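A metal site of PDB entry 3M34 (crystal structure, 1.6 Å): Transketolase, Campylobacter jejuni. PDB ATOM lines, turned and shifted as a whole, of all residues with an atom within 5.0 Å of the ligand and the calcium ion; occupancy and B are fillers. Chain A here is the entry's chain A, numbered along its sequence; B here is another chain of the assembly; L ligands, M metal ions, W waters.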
ATOM      1  N   ALA A  34      -4.011  22.077   1.628  1.00  0.00           N
ATOM      2  CA  ALA A  34      -3.092  21.417   0.701  1.00  0.00           C
ATOM      3  C   ALA A  34      -3.703  20.114   0.173  1.00  0.00           C
ATOM      4  O   ALA A  34      -3.670  19.875  -1.016  1.00  0.00           O
ATOM      5  CB  ALA A  34      -1.701  21.173   1.337  1.00  0.00           C
ATOM      6  N   HIS A  70       2.584  18.509   6.175  1.00  0.00           N
ATOM      7  CA  HIS A  70       1.322  18.917   6.740  1.00  0.00           C
ATOM      8  C   HIS A  70       0.142  18.421   5.912  1.00  0.00           C
ATOM      9  O   HIS A  70      -0.975  18.350   6.419  1.00  0.00           O
ATOM     10  CB  HIS A  70       1.262  20.436   6.962  1.00  0.00           C
ATOM     11  CG  HIS A  70       1.434  21.209   5.682  1.00  0.00           C
ATOM     12  ND1 HIS A  70       2.668  21.403   5.100  1.00  0.00           N
ATOM     13  CD2 HIS A  70       0.532  21.832   4.881  1.00  0.00           C
ATOM     14  CE1 HIS A  70       2.505  22.086   3.973  1.00  0.00           C
ATOM     15  NE2 HIS A  70       1.212  22.350   3.821  1.00  0.00           N
ATOM     16  N   GLY A 117       7.786  17.173   7.316  1.00  0.00           N
ATOM     17  CA  GLY A 117       7.208  18.074   8.320  1.00  0.00           C
ATOM     18  C   GLY A 117       8.007  19.358   8.379  1.00  0.00           C
ATOM     19  O   GLY A 117       7.484  20.430   7.980  1.00  0.00           O
ATOM     20  N   PRO A 118       9.277  19.241   8.752  1.00  0.00           N
ATOM     21  CA  PRO A 118      10.157  20.415   8.646  1.00  0.00           C
ATOM     22  C   PRO A 118      10.348  20.749   7.199  1.00  0.00           C
ATOM     23  O   PRO A 118      10.816  19.909   6.394  1.00  0.00           O
ATOM     24  CB  PRO A 118      11.449  19.978   9.303  1.00  0.00           C
ATOM     25  CG  PRO A 118      11.063  18.677  10.087  1.00  0.00           C
ATOM     26  CD  PRO A 118       9.972  18.075   9.281  1.00  0.00           C
ATOM     27  N   LEU A 119       9.970  21.934   6.803  1.00  0.00           N
ATOM     28  CA  LEU A 119       9.888  22.275   5.371  1.00  0.00           C
ATOM     29  C   LEU A 119      11.268  22.302   4.714  1.00  0.00           C
ATOM     30  O   LEU A 119      12.285  22.561   5.381  1.00  0.00           O
ATOM     31  CB  LEU A 119       9.186  23.633   5.200  1.00  0.00           C
ATOM     32  CG  LEU A 119       7.660  23.607   5.415  1.00  0.00           C
ATOM     33  CD1 LEU A 119       7.151  25.066   5.572  1.00  0.00           C
ATOM     34  CD2 LEU A 119       6.891  22.859   4.320  1.00  0.00           C
ATOM     35  N   GLY A 154       5.570  22.598  -1.663  1.00  0.00           N
ATOM     36  CA  GLY A 154       4.807  23.837  -1.651  1.00  0.00           C
ATOM     37  C   GLY A 154       5.696  25.040  -1.573  1.00  0.00           C
ATOM     38  O   GLY A 154       6.922  24.928  -1.622  1.00  0.00           O
ATOM     39  N   ASP A 155       5.085  26.185  -1.376  1.00  0.00           N
ATOM     40  CA  ASP A 155       5.850  27.436  -1.289  1.00  0.00           C
ATOM     41  C   ASP A 155       6.866  27.405  -0.181  1.00  0.00           C
ATOM     42  O   ASP A 155       7.983  27.941  -0.297  1.00  0.00           O
ATOM     43  CB  ASP A 155       4.899  28.572  -1.031  1.00  0.00           C
ATOM     44  CG  ASP A 155       3.915  28.770  -2.181  1.00  0.00           C
ATOM     45  OD1 ASP A 155       4.335  29.157  -3.286  1.00  0.00           O
ATOM     46  OD2 ASP A 155       2.680  28.596  -1.981  1.00  0.00           O
ATOM     47  N   GLY A 156       6.476  26.832   0.931  1.00  0.00           N
ATOM     48  CA  GLY A 156       7.341  26.849   2.072  1.00  0.00           C
ATOM     49  C   GLY A 156       8.631  26.079   1.811  1.00  0.00           C
ATOM     50  O   GLY A 156       9.725  26.470   2.243  1.00  0.00           O
ATOM     51  N   ASP A 157       8.498  24.916   1.168  1.00  0.00           N
ATOM     52  CA  ASP A 157       9.657  24.125   0.813  1.00  0.00           C
ATOM     53  C   ASP A 157      10.647  24.934  -0.036  1.00  0.00           C
ATOM     54  O   ASP A 157      11.843  24.871   0.173  1.00  0.00           O
ATOM     55  CB  ASP A 157       9.239  22.859   0.063  1.00  0.00           C
ATOM     56  CG  ASP A 157       8.420  21.960   0.907  1.00  0.00           C
ATOM     57  OD1 ASP A 157       8.985  21.361   1.883  1.00  0.00           O
ATOM     58  OD2 ASP A 157       7.223  21.771   0.597  1.00  0.00           O
ATOM     59  N   GLU A 160      12.841  27.653   1.598  1.00  0.00           N
ATOM     60  CA  GLU A 160      13.960  27.208   2.453  1.00  0.00           C
ATOM     61  C   GLU A 160      15.255  27.017   1.662  1.00  0.00           C
ATOM     62  O   GLU A 160      15.254  26.461   0.556  1.00  0.00           O
ATOM     63  CB  GLU A 160      13.577  25.903   3.130  1.00  0.00           C
ATOM     64  CG  GLU A 160      12.534  26.029   4.195  1.00  0.00           C
ATOM     65  CD  GLU A 160      13.097  26.632   5.506  1.00  0.00           C
ATOM     66  OE1 GLU A 160      14.290  26.948   5.549  1.00  0.00           O
ATOM     67  OE2 GLU A 160      12.331  26.802   6.465  1.00  0.00           O
ATOM     68  N   ASP A 183       3.349  22.713  -5.840  1.00  0.00           N
ATOM     69  CA  ASP A 183       2.001  23.215  -5.604  1.00  0.00           C
ATOM     70  C   ASP A 183       2.026  24.739  -5.423  1.00  0.00           C
ATOM     71  O   ASP A 183       2.279  25.254  -4.338  1.00  0.00           O
ATOM     72  CB  ASP A 183       1.365  22.542  -4.374  1.00  0.00           C
ATOM     73  CG  ASP A 183      -0.067  22.944  -4.156  1.00  0.00           C
ATOM     74  OD1 ASP A 183      -0.576  23.669  -5.050  1.00  0.00           O
ATOM     75  OD2 ASP A 183      -0.669  22.569  -3.097  1.00  0.00           O
ATOM     76  N   ASN A 185       0.077  27.739  -5.032  1.00  0.00           N
ATOM     77  CA  ASN A 185      -1.264  28.206  -4.702  1.00  0.00           C
ATOM     78  C   ASN A 185      -1.359  29.659  -4.222  1.00  0.00           C
ATOM     79  O   ASN A 185      -2.423  30.113  -3.837  1.00  0.00           O
ATOM     80  CB  ASN A 185      -1.963  27.206  -3.775  1.00  0.00           C
ATOM     81  CG  ASN A 185      -1.299  27.079  -2.440  1.00  0.00           C
ATOM     82  OD1 ASN A 185      -0.510  27.962  -2.010  1.00  0.00           O
ATOM     83  ND2 ASN A 185      -1.635  25.983  -1.710  1.00  0.00           N
ATOM     84  N   ASN A 186      -0.214  30.347  -4.236  1.00  0.00           N
ATOM     85  CA  ASN A 186      -0.111  31.752  -3.878  1.00  0.00           C
ATOM     86  C   ASN A 186      -0.470  32.075  -2.425  1.00  0.00           C
ATOM     87  O   ASN A 186      -0.648  33.243  -2.108  1.00  0.00           O
ATOM     88  CB  ASN A 186      -0.942  32.652  -4.798  1.00  0.00           C
ATOM     89  CG  ASN A 186      -0.545  34.121  -4.689  1.00  0.00           C
ATOM     90  OD1 ASN A 186      -1.408  35.012  -4.479  1.00  0.00           O
ATOM     91  ND2 ASN A 186       0.758  34.386  -4.778  1.00  0.00           N
ATOM     92  N   ILE A 187      -0.572  31.058  -1.556  1.00  0.00           N
ATOM     93  CA  ILE A 187      -0.982  31.260  -0.173  1.00  0.00           C
ATOM     94  C   ILE A 187      -0.026  30.605   0.800  1.00  0.00           C
ATOM     95  O   ILE A 187       0.456  29.490   0.544  1.00  0.00           O
ATOM     96  CB  ILE A 187      -2.413  30.657   0.036  1.00  0.00           C
ATOM     97  CG1 ILE A 187      -3.442  31.529  -0.742  1.00  0.00           C
ATOM     98  CG2 ILE A 187      -2.709  30.421   1.545  1.00  0.00           C
ATOM     99  CD1 ILE A 187      -3.686  32.877  -0.126  1.00  0.00           C
ATOM    100  N   SER A 188       0.293  31.332   1.873  1.00  0.00           N
ATOM    101  CA  SER A 188       1.026  30.740   3.018  1.00  0.00           C
ATOM    102  C   SER A 188       0.342  31.175   4.302  1.00  0.00           C
ATOM    103  O   SER A 188      -0.748  31.730   4.269  1.00  0.00           O
ATOM    104  CB  SER A 188       2.548  31.071   2.951  1.00  0.00           C
ATOM    105  OG  SER A 188       2.738  32.413   3.239  1.00  0.00           O
ATOM    106  N   ILE A 189       0.938  30.896   5.477  1.00  0.00           N
ATOM    107  CA  ILE A 189       0.239  31.218   6.721  1.00  0.00           C
ATOM    108  C   ILE A 189       0.003  32.725   6.879  1.00  0.00           C
ATOM    109  O   ILE A 189      -1.021  33.139   7.405  1.00  0.00           O
ATOM    110  CB  ILE A 189       0.998  30.622   7.924  1.00  0.00           C
ATOM    111  CG1 ILE A 189       0.858  29.088   7.900  1.00  0.00           C
ATOM    112  CG2 ILE A 189       0.500  31.179   9.219  1.00  0.00           C
ATOM    113  CD1 ILE A 189       1.698  28.415   8.956  1.00  0.00           C
ATOM    114  N   VAL A 193       1.527  34.928  -0.875  1.00  0.00           N
ATOM    115  CA  VAL A 193       2.958  34.554  -0.939  1.00  0.00           C
ATOM    116  C   VAL A 193       3.768  35.732  -1.433  1.00  0.00           C
ATOM    117  O   VAL A 193       4.910  35.886  -1.083  1.00  0.00           O
ATOM    118  CB  VAL A 193       3.137  33.333  -1.867  1.00  0.00           C
ATOM    119  CG1 VAL A 193       4.576  33.262  -2.453  1.00  0.00           C
ATOM    120  CG2 VAL A 193       2.825  32.086  -1.046  1.00  0.00           C
ATOM    121  N   ILE A 245      -5.762  26.734  -3.149  1.00  0.00           N
ATOM    122  CA  ILE A 245      -5.802  26.092  -1.859  1.00  0.00           C
ATOM    123  C   ILE A 245      -7.279  25.813  -1.480  1.00  0.00           C
ATOM    124  O   ILE A 245      -8.152  26.614  -1.723  1.00  0.00           O
ATOM    125  CB  ILE A 245      -5.003  26.887  -0.796  1.00  0.00           C
ATOM    126  CG1 ILE A 245      -4.734  26.000   0.439  1.00  0.00           C
ATOM    127  CG2 ILE A 245      -5.752  28.128  -0.314  1.00  0.00           C
ATOM    128  CD1 ILE A 245      -3.826  26.663   1.483  1.00  0.00           C
ATOM    129  N   HIS A 259      -5.430  26.754   5.537  1.00  0.00           N
ATOM    130  CA  HIS A 259      -4.129  26.098   5.557  1.00  0.00           C
ATOM    131  C   HIS A 259      -4.062  25.072   6.674  1.00  0.00           C
ATOM    132  O   HIS A 259      -3.597  23.945   6.468  1.00  0.00           O
ATOM    133  CB  HIS A 259      -2.988  27.120   5.720  1.00  0.00           C
ATOM    134  CG  HIS A 259      -1.709  26.514   6.196  1.00  0.00           C
ATOM    135  ND1 HIS A 259      -0.832  25.860   5.360  1.00  0.00           N
ATOM    136  CD2 HIS A 259      -1.205  26.369   7.452  1.00  0.00           C
ATOM    137  CE1 HIS A 259       0.158  25.355   6.078  1.00  0.00           C
ATOM    138  NE2 HIS A 259      -0.060  25.618   7.350  1.00  0.00           N
ATOM    139  N   ALA B 366       9.054  34.050  10.456  1.00  0.00           N
ATOM    140  CA  ALA B 366       9.274  33.295   9.266  1.00  0.00           C
ATOM    141  C   ALA B 366       7.992  32.602   8.836  1.00  0.00           C
ATOM    142  O   ALA B 366       7.824  31.413   9.006  1.00  0.00           O
ATOM    143  CB  ALA B 366      10.426  32.279   9.455  1.00  0.00           C
ATOM    144  N   ASP B 367       7.087  33.406   8.263  1.00  0.00           N
ATOM    145  CA  ASP B 367       5.747  32.998   7.825  1.00  0.00           C
ATOM    146  C   ASP B 367       4.804  32.590   8.948  1.00  0.00           C
ATOM    147  O   ASP B 367       3.779  32.024   8.647  1.00  0.00           O
ATOM    148  CB  ASP B 367       5.766  31.928   6.740  1.00  0.00           C
ATOM    149  CG  ASP B 367       4.414  31.777   6.010  1.00  0.00           C
ATOM    150  OD1 ASP B 367       3.809  32.825   5.615  1.00  0.00           O
ATOM    151  OD2 ASP B 367       3.913  30.649   5.873  1.00  0.00           O
ATOM    152  N   LEU B 368       5.141  32.812  10.234  1.00  0.00           N
ATOM    153  CA  LEU B 368       4.288  32.337  11.306  1.00  0.00           C
ATOM    154  C   LEU B 368       3.738  33.440  12.226  1.00  0.00           C
ATOM    155  O   LEU B 368       3.300  33.174  13.368  1.00  0.00           O
ATOM    156  CB  LEU B 368       5.021  31.305  12.171  1.00  0.00           C
ATOM    157  CG  LEU B 368       5.286  29.997  11.469  1.00  0.00           C
ATOM    158  CD1 LEU B 368       6.339  29.202  12.266  1.00  0.00           C
ATOM    159  CD2 LEU B 368       3.996  29.205  11.378  1.00  0.00           C
ATOM    160  N   ILE B 392       9.490  31.745   4.550  1.00  0.00           N
ATOM    161  CA  ILE B 392       9.930  30.539   5.215  1.00  0.00           C
ATOM    162  C   ILE B 392      11.477  30.427   5.094  1.00  0.00           C
ATOM    163  O   ILE B 392      12.017  29.576   4.361  1.00  0.00           O
ATOM    164  CB  ILE B 392       9.171  29.275   4.706  1.00  0.00           C
ATOM    165  CG1 ILE B 392       7.641  29.410   4.841  1.00  0.00           C
ATOM    166  CG2 ILE B 392       9.613  28.048   5.584  1.00  0.00           C
ATOM    167  CD1 ILE B 392       6.954  30.262   3.732  1.00  0.00           C
ATOM    168  N   GLU B 394      14.086  30.889   7.971  1.00  0.00           N
ATOM    169  CA  GLU B 394      14.447  31.148   9.358  1.00  0.00           C
ATOM    170  C   GLU B 394      15.917  31.609   9.439  1.00  0.00           C
ATOM    171  O   GLU B 394      16.233  32.529  10.210  1.00  0.00           O
ATOM    172  CB  GLU B 394      14.284  29.904  10.244  1.00  0.00           C
ATOM    173  CG  GLU B 394      12.917  29.379  10.405  1.00  0.00           C
ATOM    174  CD  GLU B 394      12.420  28.520   9.286  1.00  0.00           C
ATOM    175  OE1 GLU B 394      13.236  28.154   8.381  1.00  0.00           O
ATOM    176  OE2 GLU B 394      11.234  28.173   9.369  1.00  0.00           O
ATOM    177  N   THR B 416       9.968  32.328  15.277  1.00  0.00           N
ATOM    178  CA  THR B 416       9.521  31.112  14.659  1.00  0.00           C
ATOM    179  C   THR B 416       9.041  30.151  15.790  1.00  0.00           C
ATOM    180  O   THR B 416       9.131  30.475  16.957  1.00  0.00           O
ATOM    181  CB  THR B 416      10.588  30.421  13.737  1.00  0.00           C
ATOM    182  OG1 THR B 416      10.034  29.258  13.053  1.00  0.00           O
ATOM    183  CG2 THR B 416      11.929  30.137  14.483  1.00  0.00           C
ATOM    184  N   PHE B 417       8.637  28.948  15.390  1.00  0.00           N
ATOM    185  CA  PHE B 417       8.414  27.859  16.389  1.00  0.00           C
ATOM    186  C   PHE B 417       9.758  27.432  16.960  1.00  0.00           C
ATOM    187  O   PHE B 417      10.807  27.375  16.290  1.00  0.00           O
ATOM    188  CB  PHE B 417       7.770  26.589  15.802  1.00  0.00           C
ATOM    189  CG  PHE B 417       6.352  26.760  15.253  1.00  0.00           C
ATOM    190  CD1 PHE B 417       5.447  27.677  15.811  1.00  0.00           C
ATOM    191  CD2 PHE B 417       5.926  25.968  14.176  1.00  0.00           C
ATOM    192  CE1 PHE B 417       4.155  27.799  15.306  1.00  0.00           C
ATOM    193  CE2 PHE B 417       4.626  26.088  13.650  1.00  0.00           C
ATOM    194  CZ  PHE B 417       3.736  27.010  14.249  1.00  0.00           C
ATOM    195  N   PHE B 420      11.939  25.013  15.123  1.00  0.00           N
ATOM    196  CA  PHE B 420      12.662  25.546  13.978  1.00  0.00           C
ATOM    197  C   PHE B 420      13.676  26.577  14.296  1.00  0.00           C
ATOM    198  O   PHE B 420      14.399  27.097  13.389  1.00  0.00           O
ATOM    199  CB  PHE B 420      11.714  25.908  12.849  1.00  0.00           C
ATOM    200  CG  PHE B 420      10.780  24.768  12.481  1.00  0.00           C
ATOM    201  CD1 PHE B 420      11.294  23.500  12.303  1.00  0.00           C
ATOM    202  CD2 PHE B 420       9.430  24.933  12.403  1.00  0.00           C
ATOM    203  CE1 PHE B 420      10.479  22.442  11.995  1.00  0.00           C
ATOM    204  CE2 PHE B 420       8.610  23.890  12.089  1.00  0.00           C
ATOM    205  CZ  PHE B 420       9.161  22.623  11.917  1.00  0.00           C
ATOM    206  N   TYR B 423      16.955  25.724  12.581  1.00  0.00           N
ATOM    207  CA  TYR B 423      17.238  26.220  11.231  1.00  0.00           C
ATOM    208  C   TYR B 423      18.037  27.504  11.290  1.00  0.00           C
ATOM    209  O   TYR B 423      18.763  27.794  10.339  1.00  0.00           O
ATOM    210  CB  TYR B 423      15.977  26.438  10.393  1.00  0.00           C
ATOM    211  CG  TYR B 423      15.385  25.227   9.711  1.00  0.00           C
ATOM    212  CD1 TYR B 423      14.855  24.167  10.433  1.00  0.00           C
ATOM    213  CD2 TYR B 423      15.223  25.205   8.324  1.00  0.00           C
ATOM    214  CE1 TYR B 423      14.291  23.105   9.810  1.00  0.00           C
ATOM    215  CE2 TYR B 423      14.666  24.117   7.693  1.00  0.00           C
ATOM    216  CZ  TYR B 423      14.169  23.094   8.421  1.00  0.00           C
ATOM    217  OH  TYR B 423      13.579  22.017   7.776  1.00  0.00           O
ATOM    218  N   HIS B 456       7.490  18.402  15.414  1.00  0.00           N
ATOM    219  CA  HIS B 456       7.110  19.776  15.782  1.00  0.00           C
ATOM    220  C   HIS B 456       7.179  19.996  17.288  1.00  0.00           C
ATOM    221  O   HIS B 456       6.702  21.026  17.771  1.00  0.00           O
ATOM    222  CB  HIS B 456       5.736  20.082  15.255  1.00  0.00           C
ATOM    223  CG  HIS B 456       5.730  20.328  13.777  1.00  0.00           C
ATOM    224  ND1 HIS B 456       5.279  21.508  13.211  1.00  0.00           N
ATOM    225  CD2 HIS B 456       6.061  19.519  12.756  1.00  0.00           C
ATOM    226  CE1 HIS B 456       5.418  21.418  11.903  1.00  0.00           C
ATOM    227  NE2 HIS B 456       5.891  20.223  11.604  1.00  0.00           N
HETATM  228  N1  LIG L   1       9.410  26.196   9.171  1.00  0.00           N
HETATM  229  C1  LIG L   1       9.836  24.946   8.811  1.00  0.00           C
HETATM  230  C2  LIG L   1      11.327  24.675   8.590  1.00  0.00           C
HETATM  231  N2  LIG L   1       8.941  23.930   8.765  1.00  0.00           N
HETATM  232  C3  LIG L   1       7.643  24.150   9.020  1.00  0.00           C
HETATM  233  N3  LIG L   1       6.772  23.130   8.980  1.00  0.00           N
HETATM  234  C4  LIG L   1       7.164  25.452   9.338  1.00  0.00           C
HETATM  235  C5  LIG L   1       8.126  26.443   9.422  1.00  0.00           C
HETATM  236  C6  LIG L   1       5.692  25.770   9.622  1.00  0.00           C
HETATM  237  N4  LIG L   1       4.897  25.722   8.369  1.00  0.00           N
HETATM  238  C7  LIG L   1       4.152  24.643   8.015  1.00  0.00           C
HETATM  239  S1  LIG L   1       3.474  24.883   6.452  1.00  0.00           S
HETATM  240  C8  LIG L   1       3.976  26.533   6.410  1.00  0.00           C
HETATM  241  C9  LIG L   1       4.805  26.749   7.496  1.00  0.00           C
HETATM  242  C10 LIG L   1       5.465  28.087   7.756  1.00  0.00           C
HETATM  243  C11 LIG L   1       3.604  27.377   5.228  1.00  0.00           C
HETATM  244  C12 LIG L   1       3.891  26.466   4.081  1.00  0.00           C
HETATM  245  O1  LIG L   1       3.117  26.836   3.099  1.00  0.00           O
HETATM  246  P1  LIG L   1       2.951  25.991   1.922  1.00  0.00           P
HETATM  247  O2  LIG L   1       2.881  27.276   1.170  1.00  0.00           O
HETATM  248  O3  LIG L   1       4.253  25.332   1.952  1.00  0.00           O
HETATM  249  O4  LIG L   1       1.771  25.401   2.543  1.00  0.00           O
HETATM  250  P2  LIG L   1       0.288  25.287   1.902  1.00  0.00           P
HETATM  251  O5  LIG L   1      -0.229  26.417   2.763  1.00  0.00           O
HETATM  252  O6  LIG L   1       0.041  26.051   0.567  1.00  0.00           O
HETATM  253  O7  LIG L   1      -0.537  24.240   2.382  1.00  0.00           O
HETATM  254 CA    CA M   1       1.231  27.589  -0.491  1.00  0.00          CA
HETATM  255  O   HOH W   1       1.856  25.617  -1.674  1.00  0.00           O
HETATM  256  O   HOH W   2      -2.598  23.198   3.928  1.00  0.00           O
HETATM  257  O   HOH W   3       3.864  21.538   9.276  1.00  0.00           O
HETATM  258  O   HOH W   4       4.576  22.617   1.645  1.00  0.00           O
HETATM  259  O   HOH W   5       9.121  29.375  10.586  1.00  0.00           O
HETATM  260  O   HOH W   6       0.966  23.207  -0.823  1.00  0.00           O
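Water W1 bridges O of Asp 183 (2.7 Å) and N of Asp 155 (3.3 Å). Water W4 lies within hydrogen-bond range of an oxygen (O3) of the ligand (2.8 Å), the side-chain carboxylate (OD2) of Asp 157 (3.0 Å) and the backbone NH (N) of Gly 154 (3.5 Å). Water W2 lies within hydrogen-bond range of an oxygen (O7) of the ligand (2.8 Å), the backbone carbonyl oxygen (O) of His 259 (2.8 Å) and the backbone NH (N) of Ala 34 (2.9 Å). Water W3 lies within hydrogen-bond range of N3 of the ligand (3.3 Å) and NE2 of His 456 of chain B (3.4 Å).
The calcium ion is bound by an oxygen (O6) of the ligand, the backbone carbonyl oxygen of Ile 187, the side-chain carboxylate of Asp 155, the side-chain amide oxygen of Asn 185, an oxygen (O2) of the ligand and water W1.
N of Gly 156 sits at hydrogen-bond distance from O3 of the ligand, 2.9 Å away. N3 of the ligand lies within hydrogen-bond range of O of Gly 117 (3.0 Å). The side-chain carboxylate (OE2) of Glu 394 of chain B lies within hydrogen-bond range of a nitrogen (N1) of the ligand, 2.7 Å away. O7 of the ligand sits at hydrogen-bond distance from NE2 of His 70, 2.9 Å away. A ring nitrogen (ND1) of His 259 sits at hydrogen-bond distance from an oxygen (O5) of the ligand (2.7 Å). N of Leu 119 is in hydrogen-bond range of N2 of the ligand (3.0 Å).
Ala 34 touches the ligand. CA of Pro 118 touches N2 of the ligand (3.7 Å). Gly 154 touches the ligand (C to O3, 3.8 Å). Glu 160 touches the ligand. Ile 189 touches the ligand (CD1 to C9, 3.8 Å). CD1 of Ile 245 touches O5 of the ligand, 3.8 Å away. Asp 367 of chain B touches the ligand (OD2 to C11, 3.3 Å). Ile 392 of chain B touches the ligand (CG1 to C10, 3.9 Å). CE2 of Phe 420 of chain B touches C3 of the ligand (3.2 Å). Tyr 423 of chain B touches the ligand (CZ to C2, 3.3 Å). CE1 of His 456 of chain B touches N3 of the ligand, 3.6 Å away. Hydrophobic or aromatic side chains that line the ligand: Ala 34, His 70, Leu 119, Ile 189, Ile 245, His 259, Ile 392 of chain B, Phe 420 of chain B, Tyr 423 of chain B and His 456 of chain B. 20 residues have an atom within 4 Å of the ligand: Ala 34, His 70, Gly 117, Pro 118, Leu 119, Gly 154, Asp 155, Gly 156, Glu 160, Asn 185, Ile 187, Ile 189, Ile 245, His 259, Asp 367 of chain B, Ile 392 of chain B, Glu 394 of chain B, Phe 420 of chain B, Tyr 423 of chain B and His 456 of chain B.
The backbone NH (N) of Glu 160 lies close to the backbone carbonyl oxygen (O) of Ile 392 of chain B (3.5 Å). OD2 of Asp 367 of chain B is in hydrogen-bond range of N of Ile 189, 3.0 Å away. The side-chain carboxylate (OE2) of Glu 160 lies close to the side-chain carboxylate (OE1) of Glu 394 of chain B, at 2.5 Å. The side-chain hydroxyl (OH) of Tyr 423 of chain B is in hydrogen-bond range of the backbone carbonyl oxygen (O) of Leu 119 (2.8 Å). The side-chain carboxylate (OD2) of Asp 157 is in hydrogen-bond range of the backbone NH (N) of Gly 154 (2.9 Å). OG of Ser 188 sits at hydrogen-bond distance from OD1 of Asp 367 of chain B, 2.6 Å away.
Within 4 Å of the calcium ion: Asp 155, Asn 185 and Ile 187. The nearest printed residue that does not touch the calcium ion is Ser 188 (4.5 Å).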
